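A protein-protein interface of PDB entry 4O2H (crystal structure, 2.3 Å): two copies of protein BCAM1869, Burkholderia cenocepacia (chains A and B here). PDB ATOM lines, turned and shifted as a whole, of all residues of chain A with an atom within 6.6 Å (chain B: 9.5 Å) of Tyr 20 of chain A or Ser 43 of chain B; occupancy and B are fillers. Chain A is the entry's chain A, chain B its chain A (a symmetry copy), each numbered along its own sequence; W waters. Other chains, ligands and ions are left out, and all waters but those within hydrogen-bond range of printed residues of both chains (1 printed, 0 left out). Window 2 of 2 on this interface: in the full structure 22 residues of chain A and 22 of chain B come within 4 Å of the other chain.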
ATOM      1  N   GLY A  14      17.035  19.297 -10.197  1.00  0.00           N
ATOM      2  CA  GLY A  14      16.573  18.065  -9.601  1.00  0.00           C
ATOM      3  C   GLY A  14      16.061  18.424  -8.219  1.00  0.00           C
ATOM      4  O   GLY A  14      16.083  19.600  -7.813  1.00  0.00           O
ATOM      5  N   PRO A  15      15.598  17.435  -7.449  1.00  0.00           N
ATOM      6  CA  PRO A  15      15.185  17.727  -6.069  1.00  0.00           C
ATOM      7  C   PRO A  15      16.333  18.287  -5.211  1.00  0.00           C
ATOM      8  O   PRO A  15      17.508  18.231  -5.604  1.00  0.00           O
ATOM      9  CB  PRO A  15      14.787  16.326  -5.530  1.00  0.00           C
ATOM     10  CG  PRO A  15      14.570  15.470  -6.720  1.00  0.00           C
ATOM     11  CD  PRO A  15      15.533  15.983  -7.740  1.00  0.00           C
ATOM     12  N   SER A  16      15.995  18.742  -3.994  1.00  0.00           N
ATOM     13  CA  SER A  16      16.970  19.084  -2.975  1.00  0.00           C
ATOM     14  C   SER A  16      17.750  17.800  -2.623  1.00  0.00           C
ATOM     15  O   SER A  16      17.231  16.719  -2.894  1.00  0.00           O
ATOM     16  CB  SER A  16      16.271  19.621  -1.729  1.00  0.00           C
ATOM     17  OG  SER A  16      15.514  20.783  -2.003  1.00  0.00           O
ATOM     18  N   PRO A  17      18.955  17.870  -1.990  1.00  0.00           N
ATOM     19  CA  PRO A  17      19.709  16.632  -1.690  1.00  0.00           C
ATOM     20  C   PRO A  17      18.909  15.593  -0.879  1.00  0.00           C
ATOM     21  O   PRO A  17      19.152  14.400  -1.030  1.00  0.00           O
ATOM     22  CB  PRO A  17      20.931  17.149  -0.891  1.00  0.00           C
ATOM     23  CG  PRO A  17      21.126  18.529  -1.353  1.00  0.00           C
ATOM     24  CD  PRO A  17      19.738  19.075  -1.635  1.00  0.00           C
ATOM     25  N   ASP A  18      17.921  16.030  -0.067  1.00  0.00           N
ATOM     26  CA  ASP A  18      17.078  15.120   0.726  1.00  0.00           C
ATOM     27  C   ASP A  18      15.921  14.516  -0.119  1.00  0.00           C
ATOM     28  O   ASP A  18      15.138  13.738   0.412  1.00  0.00           O
ATOM     29  CB  ASP A  18      16.549  15.808   2.008  1.00  0.00           C
ATOM     30  CG  ASP A  18      15.456  16.854   1.804  1.00  0.00           C
ATOM     31  OD1 ASP A  18      15.385  17.439   0.693  1.00  0.00           O
ATOM     32  OD2 ASP A  18      14.684  17.100   2.764  1.00  0.00           O
ATOM     33  N   GLY A  19      15.853  14.834  -1.421  1.00  0.00           N
ATOM     34  CA  GLY A  19      14.867  14.253  -2.343  1.00  0.00           C
ATOM     35  C   GLY A  19      13.564  15.004  -2.575  1.00  0.00           C
ATOM     36  O   GLY A  19      12.742  14.556  -3.373  1.00  0.00           O
ATOM     37  N   TYR A  20      13.346  16.139  -1.901  1.00  0.00           N
ATOM     38  CA  TYR A  20      12.128  16.934  -2.108  1.00  0.00           C
ATOM     39  C   TYR A  20      12.378  18.127  -2.978  1.00  0.00           C
ATOM     40  O   TYR A  20      13.440  18.738  -2.869  1.00  0.00           O
ATOM     41  CB  TYR A  20      11.546  17.423  -0.777  1.00  0.00           C
ATOM     42  CG  TYR A  20      11.078  16.309   0.127  1.00  0.00           C
ATOM     43  CD1 TYR A  20       9.814  15.744  -0.028  1.00  0.00           C
ATOM     44  CD2 TYR A  20      11.887  15.835   1.161  1.00  0.00           C
ATOM     45  CE1 TYR A  20       9.346  14.764   0.849  1.00  0.00           C
ATOM     46  CE2 TYR A  20      11.458  14.799   1.998  1.00  0.00           C
ATOM     47  CZ  TYR A  20      10.179  14.275   1.840  1.00  0.00           C
ATOM     48  OH  TYR A  20       9.721  13.282   2.659  1.00  0.00           O
ATOM     49  N   VAL A  21      11.397  18.452  -3.848  1.00  0.00           N
ATOM     50  CA  VAL A  21      11.314  19.666  -4.687  1.00  0.00           C
ATOM     51  C   VAL A  21      10.641  20.721  -3.811  1.00  0.00           C
ATOM     52  O   VAL A  21       9.487  20.527  -3.433  1.00  0.00           O
ATOM     53  CB  VAL A  21      10.536  19.425  -6.030  1.00  0.00           C
ATOM     54  CG1 VAL A  21      10.295  20.749  -6.784  1.00  0.00           C
ATOM     55  CG2 VAL A  21      11.283  18.425  -6.914  1.00  0.00           C
ATOM     56  N   ARG A  22      11.348  21.791  -3.442  1.00  0.00           N
ATOM     57  CA  ARG A  22      10.803  22.804  -2.531  1.00  0.00           C
ATOM     58  C   ARG A  22      10.096  23.906  -3.271  1.00  0.00           C
ATOM     59  O   ARG A  22      10.658  24.531  -4.169  1.00  0.00           O
ATOM     60  CB  ARG A  22      11.868  23.350  -1.594  1.00  0.00           C
ATOM     61  CG  ARG A  22      12.180  22.323  -0.512  1.00  0.00           C
ATOM     62  CD  ARG A  22      13.274  22.702   0.481  1.00  0.00           C
ATOM     63  NE  ARG A  22      13.158  21.808   1.634  1.00  0.00           N
ATOM     64  CZ  ARG A  22      13.592  20.547   1.664  1.00  0.00           C
ATOM     65  NH1 ARG A  22      13.375  19.791   2.726  1.00  0.00           N
ATOM     66  NH2 ARG A  22      14.238  20.034   0.627  1.00  0.00           N
ATOM     67  N   ARG A  97       0.813  11.454  -1.696  1.00  0.00           N
ATOM     68  CA  ARG A  97       2.213  11.108  -1.780  1.00  0.00           C
ATOM     69  C   ARG A  97       2.825  11.896  -2.925  1.00  0.00           C
ATOM     70  O   ARG A  97       2.263  11.920  -4.013  1.00  0.00           O
ATOM     71  CB  ARG A  97       2.411   9.595  -1.946  1.00  0.00           C
ATOM     72  CG  ARG A  97       3.880   9.153  -1.832  1.00  0.00           C
ATOM     73  CD  ARG A  97       4.574   8.959  -3.180  1.00  0.00           C
ATOM     74  NE  ARG A  97       3.904   7.900  -3.923  1.00  0.00           N
ATOM     75  CZ  ARG A  97       3.349   8.031  -5.120  1.00  0.00           C
ATOM     76  NH1 ARG A  97       3.474   9.180  -5.804  1.00  0.00           N
ATOM     77  NH2 ARG A  97       2.729   7.004  -5.680  1.00  0.00           N
ATOM     78  N   SER A  98       3.982  12.547  -2.676  1.00  0.00           N
ATOM     79  CA  SER A  98       4.689  13.340  -3.678  1.00  0.00           C
ATOM     80  C   SER A  98       6.160  13.457  -3.361  1.00  0.00           C
ATOM     81  O   SER A  98       6.613  12.958  -2.332  1.00  0.00           O
ATOM     82  CB  SER A  98       4.087  14.746  -3.782  1.00  0.00           C
ATOM     83  OG  SER A  98       4.408  15.493  -2.621  1.00  0.00           O
ATOM     84  N   ASN A  99       6.900  14.160  -4.244  1.00  0.00           N
ATOM     85  CA  ASN A  99       8.318  14.483  -4.077  1.00  0.00           C
ATOM     86  C   ASN A  99       8.434  15.962  -3.738  1.00  0.00           C
ATOM     87  O   ASN A  99       9.470  16.577  -3.977  1.00  0.00           O
ATOM     88  CB  ASN A  99       9.133  14.112  -5.334  1.00  0.00           C
ATOM     89  CG  ASN A  99       8.828  14.927  -6.566  1.00  0.00           C
ATOM     90  OD1 ASN A  99       7.734  15.463  -6.754  1.00  0.00           O
ATOM     91  ND2 ASN A  99       9.790  14.969  -7.474  1.00  0.00           N
ATOM     92  N   VAL A 100       7.343  16.540  -3.218  1.00  0.00           N
ATOM     93  CA  VAL A 100       7.273  17.958  -2.857  1.00  0.00           C
ATOM     94  C   VAL A 100       7.341  18.185  -1.356  1.00  0.00           C
ATOM     95  O   VAL A 100       6.699  17.491  -0.581  1.00  0.00           O
ATOM     96  CB  VAL A 100       5.997  18.652  -3.426  1.00  0.00           C
ATOM     97  CG1 VAL A 100       5.861  20.116  -2.945  1.00  0.00           C
ATOM     98  CG2 VAL A 100       5.950  18.576  -4.956  1.00  0.00           C
ATOM     99  N   MET A 101       8.056  19.243  -0.974  1.00  0.00           N
ATOM    100  CA  MET A 101       8.058  19.816   0.365  1.00  0.00           C
ATOM    101  C   MET A 101       7.663  21.274   0.215  1.00  0.00           C
ATOM    102  O   MET A 101       8.358  22.045  -0.466  1.00  0.00           O
ATOM    103  CB  MET A 101       9.412  19.644   1.095  1.00  0.00           C
ATOM    104  CG  MET A 101       9.450  20.337   2.429  1.00  0.00           C
ATOM    105  SD  MET A 101       8.091  19.707   3.664  1.00  0.00           S
ATOM    106  CE  MET A 101       8.886  18.062   4.198  1.00  0.00           C
ATOM    107  N   ASP A 109      10.641  24.738   5.761  1.00  0.00           N
ATOM    108  CA  ASP A 109       9.693  23.657   5.474  1.00  0.00           C
ATOM    109  C   ASP A 109       8.448  23.785   6.334  1.00  0.00           C
ATOM    110  O   ASP A 109       8.539  24.243   7.472  1.00  0.00           O
ATOM    111  CB  ASP A 109      10.353  22.294   5.742  1.00  0.00           C
ATOM    112  CG  ASP A 109      11.470  21.926   4.785  1.00  0.00           C
ATOM    113  OD1 ASP A 109      11.712  22.695   3.827  1.00  0.00           O
ATOM    114  OD2 ASP A 109      12.066  20.839   4.961  1.00  0.00           O
ATOM    115  N   MET A 112       5.071  17.595   5.972  1.00  0.00           N
ATOM    116  CA  MET A 112       4.252  16.665   5.179  1.00  0.00           C
ATOM    117  C   MET A 112       2.773  16.997   5.168  1.00  0.00           C
ATOM    118  O   MET A 112       2.170  16.977   4.092  1.00  0.00           O
ATOM    119  CB  MET A 112       4.395  15.217   5.692  1.00  0.00           C
ATOM    120  CG  MET A 112       5.830  14.739   5.781  1.00  0.00           C
ATOM    121  SD  MET A 112       6.809  15.198   4.180  1.00  0.00           S
ATOM    122  CE  MET A 112       6.321  13.642   3.101  1.00  0.00           C
ATOM    123  N   LEU B  40       9.978   8.383  -7.851  1.00  0.00           N
ATOM    124  CA  LEU B  40      10.665   8.369  -6.573  1.00  0.00           C
ATOM    125  C   LEU B  40       9.718   8.806  -5.464  1.00  0.00           C
ATOM    126  O   LEU B  40       8.840   9.637  -5.706  1.00  0.00           O
ATOM    127  CB  LEU B  40      11.903   9.302  -6.626  1.00  0.00           C
ATOM    128  CG  LEU B  40      12.960   8.927  -7.693  1.00  0.00           C
ATOM    129  CD1 LEU B  40      14.180   9.841  -7.592  1.00  0.00           C
ATOM    130  CD2 LEU B  40      13.357   7.416  -7.634  1.00  0.00           C
ATOM    131  N   ASP B  41       9.847   8.188  -4.271  1.00  0.00           N
ATOM    132  CA  ASP B  41       9.087   8.578  -3.066  1.00  0.00           C
ATOM    133  C   ASP B  41      10.115   8.918  -1.943  1.00  0.00           C
ATOM    134  O   ASP B  41      10.533   8.005  -1.230  1.00  0.00           O
ATOM    135  CB  ASP B  41       8.065   7.480  -2.628  1.00  0.00           C
ATOM    136  CG  ASP B  41       7.202   7.860  -1.425  1.00  0.00           C
ATOM    137  OD1 ASP B  41       7.369   8.972  -0.898  1.00  0.00           O
ATOM    138  OD2 ASP B  41       6.285   7.087  -1.083  1.00  0.00           O
ATOM    139  N   PRO B  42      10.525  10.206  -1.766  1.00  0.00           N
ATOM    140  CA  PRO B  42      11.543  10.537  -0.723  1.00  0.00           C
ATOM    141  C   PRO B  42      11.065  10.258   0.713  1.00  0.00           C
ATOM    142  O   PRO B  42      11.881  10.008   1.602  1.00  0.00           O
ATOM    143  CB  PRO B  42      11.812  12.034  -0.942  1.00  0.00           C
ATOM    144  CG  PRO B  42      10.597  12.545  -1.644  1.00  0.00           C
ATOM    145  CD  PRO B  42      10.128  11.414  -2.517  1.00  0.00           C
ATOM    146  N   SER B  43       9.757  10.285   0.927  1.00  0.00           N
ATOM    147  CA  SER B  43       9.155   9.974   2.218  1.00  0.00           C
ATOM    148  C   SER B  43       9.308   8.467   2.530  1.00  0.00           C
ATOM    149  O   SER B  43       9.652   8.127   3.650  1.00  0.00           O
ATOM    150  CB  SER B  43       7.693  10.389   2.230  1.00  0.00           C
ATOM    151  OG  SER B  43       7.056   9.894   3.396  1.00  0.00           O
ATOM    152  N   LEU B  44       9.107   7.587   1.545  1.00  0.00           N
ATOM    153  CA  LEU B  44       9.328   6.152   1.692  1.00  0.00           C
ATOM    154  C   LEU B  44      10.819   5.864   1.929  1.00  0.00           C
ATOM    155  O   LEU B  44      11.149   5.073   2.820  1.00  0.00           O
ATOM    156  CB  LEU B  44       8.825   5.383   0.464  1.00  0.00           C
ATOM    157  CG  LEU B  44       9.123   3.848   0.413  1.00  0.00           C
ATOM    158  CD1 LEU B  44       8.461   3.106   1.567  1.00  0.00           C
ATOM    159  CD2 LEU B  44       8.680   3.255  -0.908  1.00  0.00           C
ATOM    160  N   LEU B  45      11.706   6.546   1.158  1.00  0.00           N
ATOM    161  CA  LEU B  45      13.154   6.398   1.237  1.00  0.00           C
ATOM    162  C   LEU B  45      13.659   6.705   2.675  1.00  0.00           C
ATOM    163  O   LEU B  45      14.454   5.933   3.221  1.00  0.00           O
ATOM    164  CB  LEU B  45      13.879   7.289   0.180  1.00  0.00           C
ATOM    165  CG  LEU B  45      15.434   7.295   0.291  1.00  0.00           C
ATOM    166  CD1 LEU B  45      16.029   5.895   0.003  1.00  0.00           C
ATOM    167  CD2 LEU B  45      16.072   8.327  -0.614  1.00  0.00           C
ATOM    168  N   ALA B  46      13.177   7.806   3.277  1.00  0.00           N
ATOM    169  CA  ALA B  46      13.558   8.152   4.649  1.00  0.00           C
ATOM    170  C   ALA B  46      13.005   7.106   5.610  1.00  0.00           C
ATOM    171  O   ALA B  46      13.679   6.732   6.574  1.00  0.00           O
ATOM    172  CB  ALA B  46      13.048   9.546   5.026  1.00  0.00           C
ATOM    173  N   GLU B  47      11.780   6.645   5.334  1.00  0.00           N
ATOM    174  CA  GLU B  47      11.061   5.674   6.124  1.00  0.00           C
ATOM    175  C   GLU B  47      11.848   4.346   6.213  1.00  0.00           C
ATOM    176  O   GLU B  47      12.038   3.841   7.314  1.00  0.00           O
ATOM    177  CB  GLU B  47       9.678   5.487   5.510  1.00  0.00           C
ATOM    178  CG  GLU B  47       8.684   4.684   6.327  1.00  0.00           C
ATOM    179  CD  GLU B  47       7.366   4.535   5.590  1.00  0.00           C
ATOM    180  OE1 GLU B  47       6.615   5.534   5.497  1.00  0.00           O
ATOM    181  OE2 GLU B  47       7.106   3.428   5.067  1.00  0.00           O
ATOM    182  N   LEU B  48      12.335   3.813   5.067  1.00  0.00           N
ATOM    183  CA  LEU B  48      13.131   2.583   4.979  1.00  0.00           C
ATOM    184  C   LEU B  48      14.474   2.748   5.707  1.00  0.00           C
ATOM    185  O   LEU B  48      14.893   1.842   6.437  1.00  0.00           O
ATOM    186  CB  LEU B  48      13.383   2.211   3.509  1.00  0.00           C
ATOM    187  CG  LEU B  48      12.195   1.751   2.644  1.00  0.00           C
ATOM    188  CD1 LEU B  48      12.542   1.817   1.212  1.00  0.00           C
ATOM    189  CD2 LEU B  48      11.787   0.315   2.936  1.00  0.00           C
ATOM    190  N   ARG B  49      15.142   3.910   5.512  1.00  0.00           N
ATOM    191  CA  ARG B  49      16.426   4.219   6.134  1.00  0.00           C
ATOM    192  C   ARG B  49      16.305   4.266   7.656  1.00  0.00           C
ATOM    193  O   ARG B  49      17.247   3.911   8.344  1.00  0.00           O
ATOM    194  CB  ARG B  49      16.981   5.549   5.612  1.00  0.00           C
ATOM    195  CG  ARG B  49      17.743   5.404   4.300  1.00  0.00           C
ATOM    196  CD  ARG B  49      18.058   6.765   3.735  1.00  0.00           C
ATOM    197  NE  ARG B  49      18.744   6.683   2.448  1.00  0.00           N
ATOM    198  CZ  ARG B  49      18.945   7.724   1.645  1.00  0.00           C
ATOM    199  NH1 ARG B  49      18.500   8.930   1.985  1.00  0.00           N
ATOM    200  NH2 ARG B  49      19.582   7.568   0.491  1.00  0.00           N
ATOM    201  N   ASP B  50      15.127   4.648   8.160  1.00  0.00           N
ATOM    202  CA  ASP B  50      14.757   4.724   9.573  1.00  0.00           C
ATOM    203  C   ASP B  50      14.574   3.329  10.171  1.00  0.00           C
ATOM    204  O   ASP B  50      14.678   3.147  11.391  1.00  0.00           O
ATOM    205  CB  ASP B  50      13.451   5.501   9.703  1.00  0.00           C
ATOM    206  CG  ASP B  50      13.478   6.503  10.820  1.00  0.00           C
ATOM    207  OD1 ASP B  50      13.664   7.707  10.528  1.00  0.00           O
ATOM    208  OD2 ASP B  50      13.318   6.089  11.992  1.00  0.00           O
ATOM    209  N   ASN B  51      14.286   2.352   9.300  1.00  0.00           N
ATOM    210  CA  ASN B  51      14.087   0.953   9.666  1.00  0.00           C
ATOM    211  C   ASN B  51      15.313   0.122   9.263  1.00  0.00           C
ATOM    212  O   ASN B  51      15.171  -1.047   8.939  1.00  0.00           O
ATOM    213  CB  ASN B  51      12.783   0.405   9.031  1.00  0.00           C
ATOM    214  CG  ASN B  51      11.563   1.210   9.396  1.00  0.00           C
ATOM    215  OD1 ASN B  51      11.499   1.845  10.459  1.00  0.00           O
ATOM    216  ND2 ASN B  51      10.572   1.219   8.515  1.00  0.00           N
ATOM    217  N   LEU B  57      17.668   4.684  -3.333  1.00  0.00           N
ATOM    218  CA  LEU B  57      16.425   5.253  -3.846  1.00  0.00           C
ATOM    219  C   LEU B  57      15.251   4.376  -3.439  1.00  0.00           C
ATOM    220  O   LEU B  57      15.424   3.167  -3.237  1.00  0.00           O
ATOM    221  CB  LEU B  57      16.435   5.344  -5.394  1.00  0.00           C
ATOM    222  CG  LEU B  57      17.480   6.163  -6.144  1.00  0.00           C
ATOM    223  CD1 LEU B  57      17.393   5.840  -7.641  1.00  0.00           C
ATOM    224  CD2 LEU B  57      17.275   7.690  -5.926  1.00  0.00           C
ATOM    225  N   ALA B  58      14.049   4.964  -3.406  1.00  0.00           N
ATOM    226  CA  ALA B  58      12.825   4.249  -3.165  1.00  0.00           C
ATOM    227  C   ALA B  58      11.720   4.906  -3.941  1.00  0.00           C
ATOM    228  O   ALA B  58      11.738   6.126  -4.142  1.00  0.00           O
ATOM    229  CB  ALA B  58      12.497   4.223  -1.683  1.00  0.00           C
ATOM    230  N   GLY B  59      10.726   4.117  -4.328  1.00  0.00           N
ATOM    231  CA  GLY B  59       9.603   4.676  -5.056  1.00  0.00           C
ATOM    232  C   GLY B  59       8.534   3.671  -5.359  1.00  0.00           C
ATOM    233  O   GLY B  59       8.538   2.549  -4.839  1.00  0.00           O
ATOM    234  N   ASP B  79       5.818  -0.880  -4.317  1.00  0.00           N
ATOM    235  CA  ASP B  79       6.907  -0.027  -3.842  1.00  0.00           C
ATOM    236  C   ASP B  79       8.199  -0.789  -3.967  1.00  0.00           C
ATOM    237  O   ASP B  79       8.250  -2.011  -3.728  1.00  0.00           O
ATOM    238  CB  ASP B  79       6.687   0.439  -2.389  1.00  0.00           C
ATOM    239  CG  ASP B  79       5.569   1.446  -2.204  1.00  0.00           C
ATOM    240  OD1 ASP B  79       5.072   1.988  -3.225  1.00  0.00           O
ATOM    241  OD2 ASP B  79       5.205   1.713  -1.048  1.00  0.00           O
HETATM  242  O   HOH W   1       6.329  10.622  -5.515  1.00  0.00           O
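No position is printed for both chains. Of the 8 pairs that touch across the chains among the printed residues, none has its exchanged pair printed and touching as well.
The side-chain hydroxyl of Tyr 20 of chain A lies close to the backbone NH of Ser 43 of chain B (3.5 Å). The side-chain carboxylate (OD2) of Asp 41 of chain B is in salt-bridge range of the guanidinium group (NE) of Arg 97 of chain A (3.8 Å).
Water W1 lies within hydrogen-bond range of the backbone carbonyl oxygen of Leu 40 of chain B and the guanidinium group of Arg 97 of chain A.
The backbone carbonyl oxygen (O) of Tyr 20 of chain A lies within hydrogen-bond range of the side-chain hydroxyl (OG) of Ser 16 of chain A, at 3.0 Å. OD1 of Asp 18 of chain A lies within salt-bridge range of NH2 of Arg 22 of chain A (2.8 Å). The side-chain hydroxyl (OG) of Ser 98 of chain A lies within hydrogen-bond range of the backbone NH (N) of Val 100 of chain A, 3.2 Å away. The side-chain carboxylate (OD1) of Asp 41 of chain B sits close to the backbone NH (N) of Ser 43 of chain B (3.3 Å). OD1 of Asp 41 of chain B is in hydrogen-bond range of N of Leu 44 of chain B (3.3 Å). N of Asp 41 of chain B is in hydrogen-bond range of O of Ala 58 of chain B (2.8 Å).
Of the 16 printed residues of chain B, 3 touch a printed residue of chain A. Printed residues of chain B that touch a printed residue of chain A: Asp 41, Pro 42 and Ser 43. Hydrophobic or aromatic side chains of chain B within 4 Å of the printed part of chain A: Pro 42. Hydrophobic or aromatic side chains of chain A that line the printed part of chain B: Tyr 20 and Met 112.
No residue of chain B comes within 4 Å of Ser 16 of chain A. Tyr 20 of chain A touches just these residues of chain B: Pro 42 and Ser 43. No residue of chain B comes within 4 Å of Val 21 of chain A. Printed residues of chain B within 4 Å of Arg 97 of chain A: Asp 41 (3.3 Å). Printed residues of chain B within 4 Å of Asn 99 of chain A: Pro 42 (3.9 Å). Of the printed residues of chain B, Met 112 of chain A touches Ser 43. Ser 43 of chain B touches two residues of chain A. The nearest residue of chain B that does not touch Tyr 20 of chain A is Ala 46 of chain B (5.5 Å). The nearest residue of chain A that does not touch Ser 43 of chain B is Ser 98 of chain A (5.3 Å).
Among the printed residues, merely in contact across the chains: Gly 19 of chain A with Pro 42 of chain B (3.4 Å), Tyr 20 of chain A with Pro 42 of chain B (3.6 Å), Met 112 of chain A with Ser 43 of chain B (3.6 Å), Ser 98 of chain A with Pro 42 of chain B (3.8 Å), Asn 99 of chain A with Pro 42 of chain B (3.9 Å) and Asp 18 of chain A with Pro 42 of chain B (3.97 Å).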
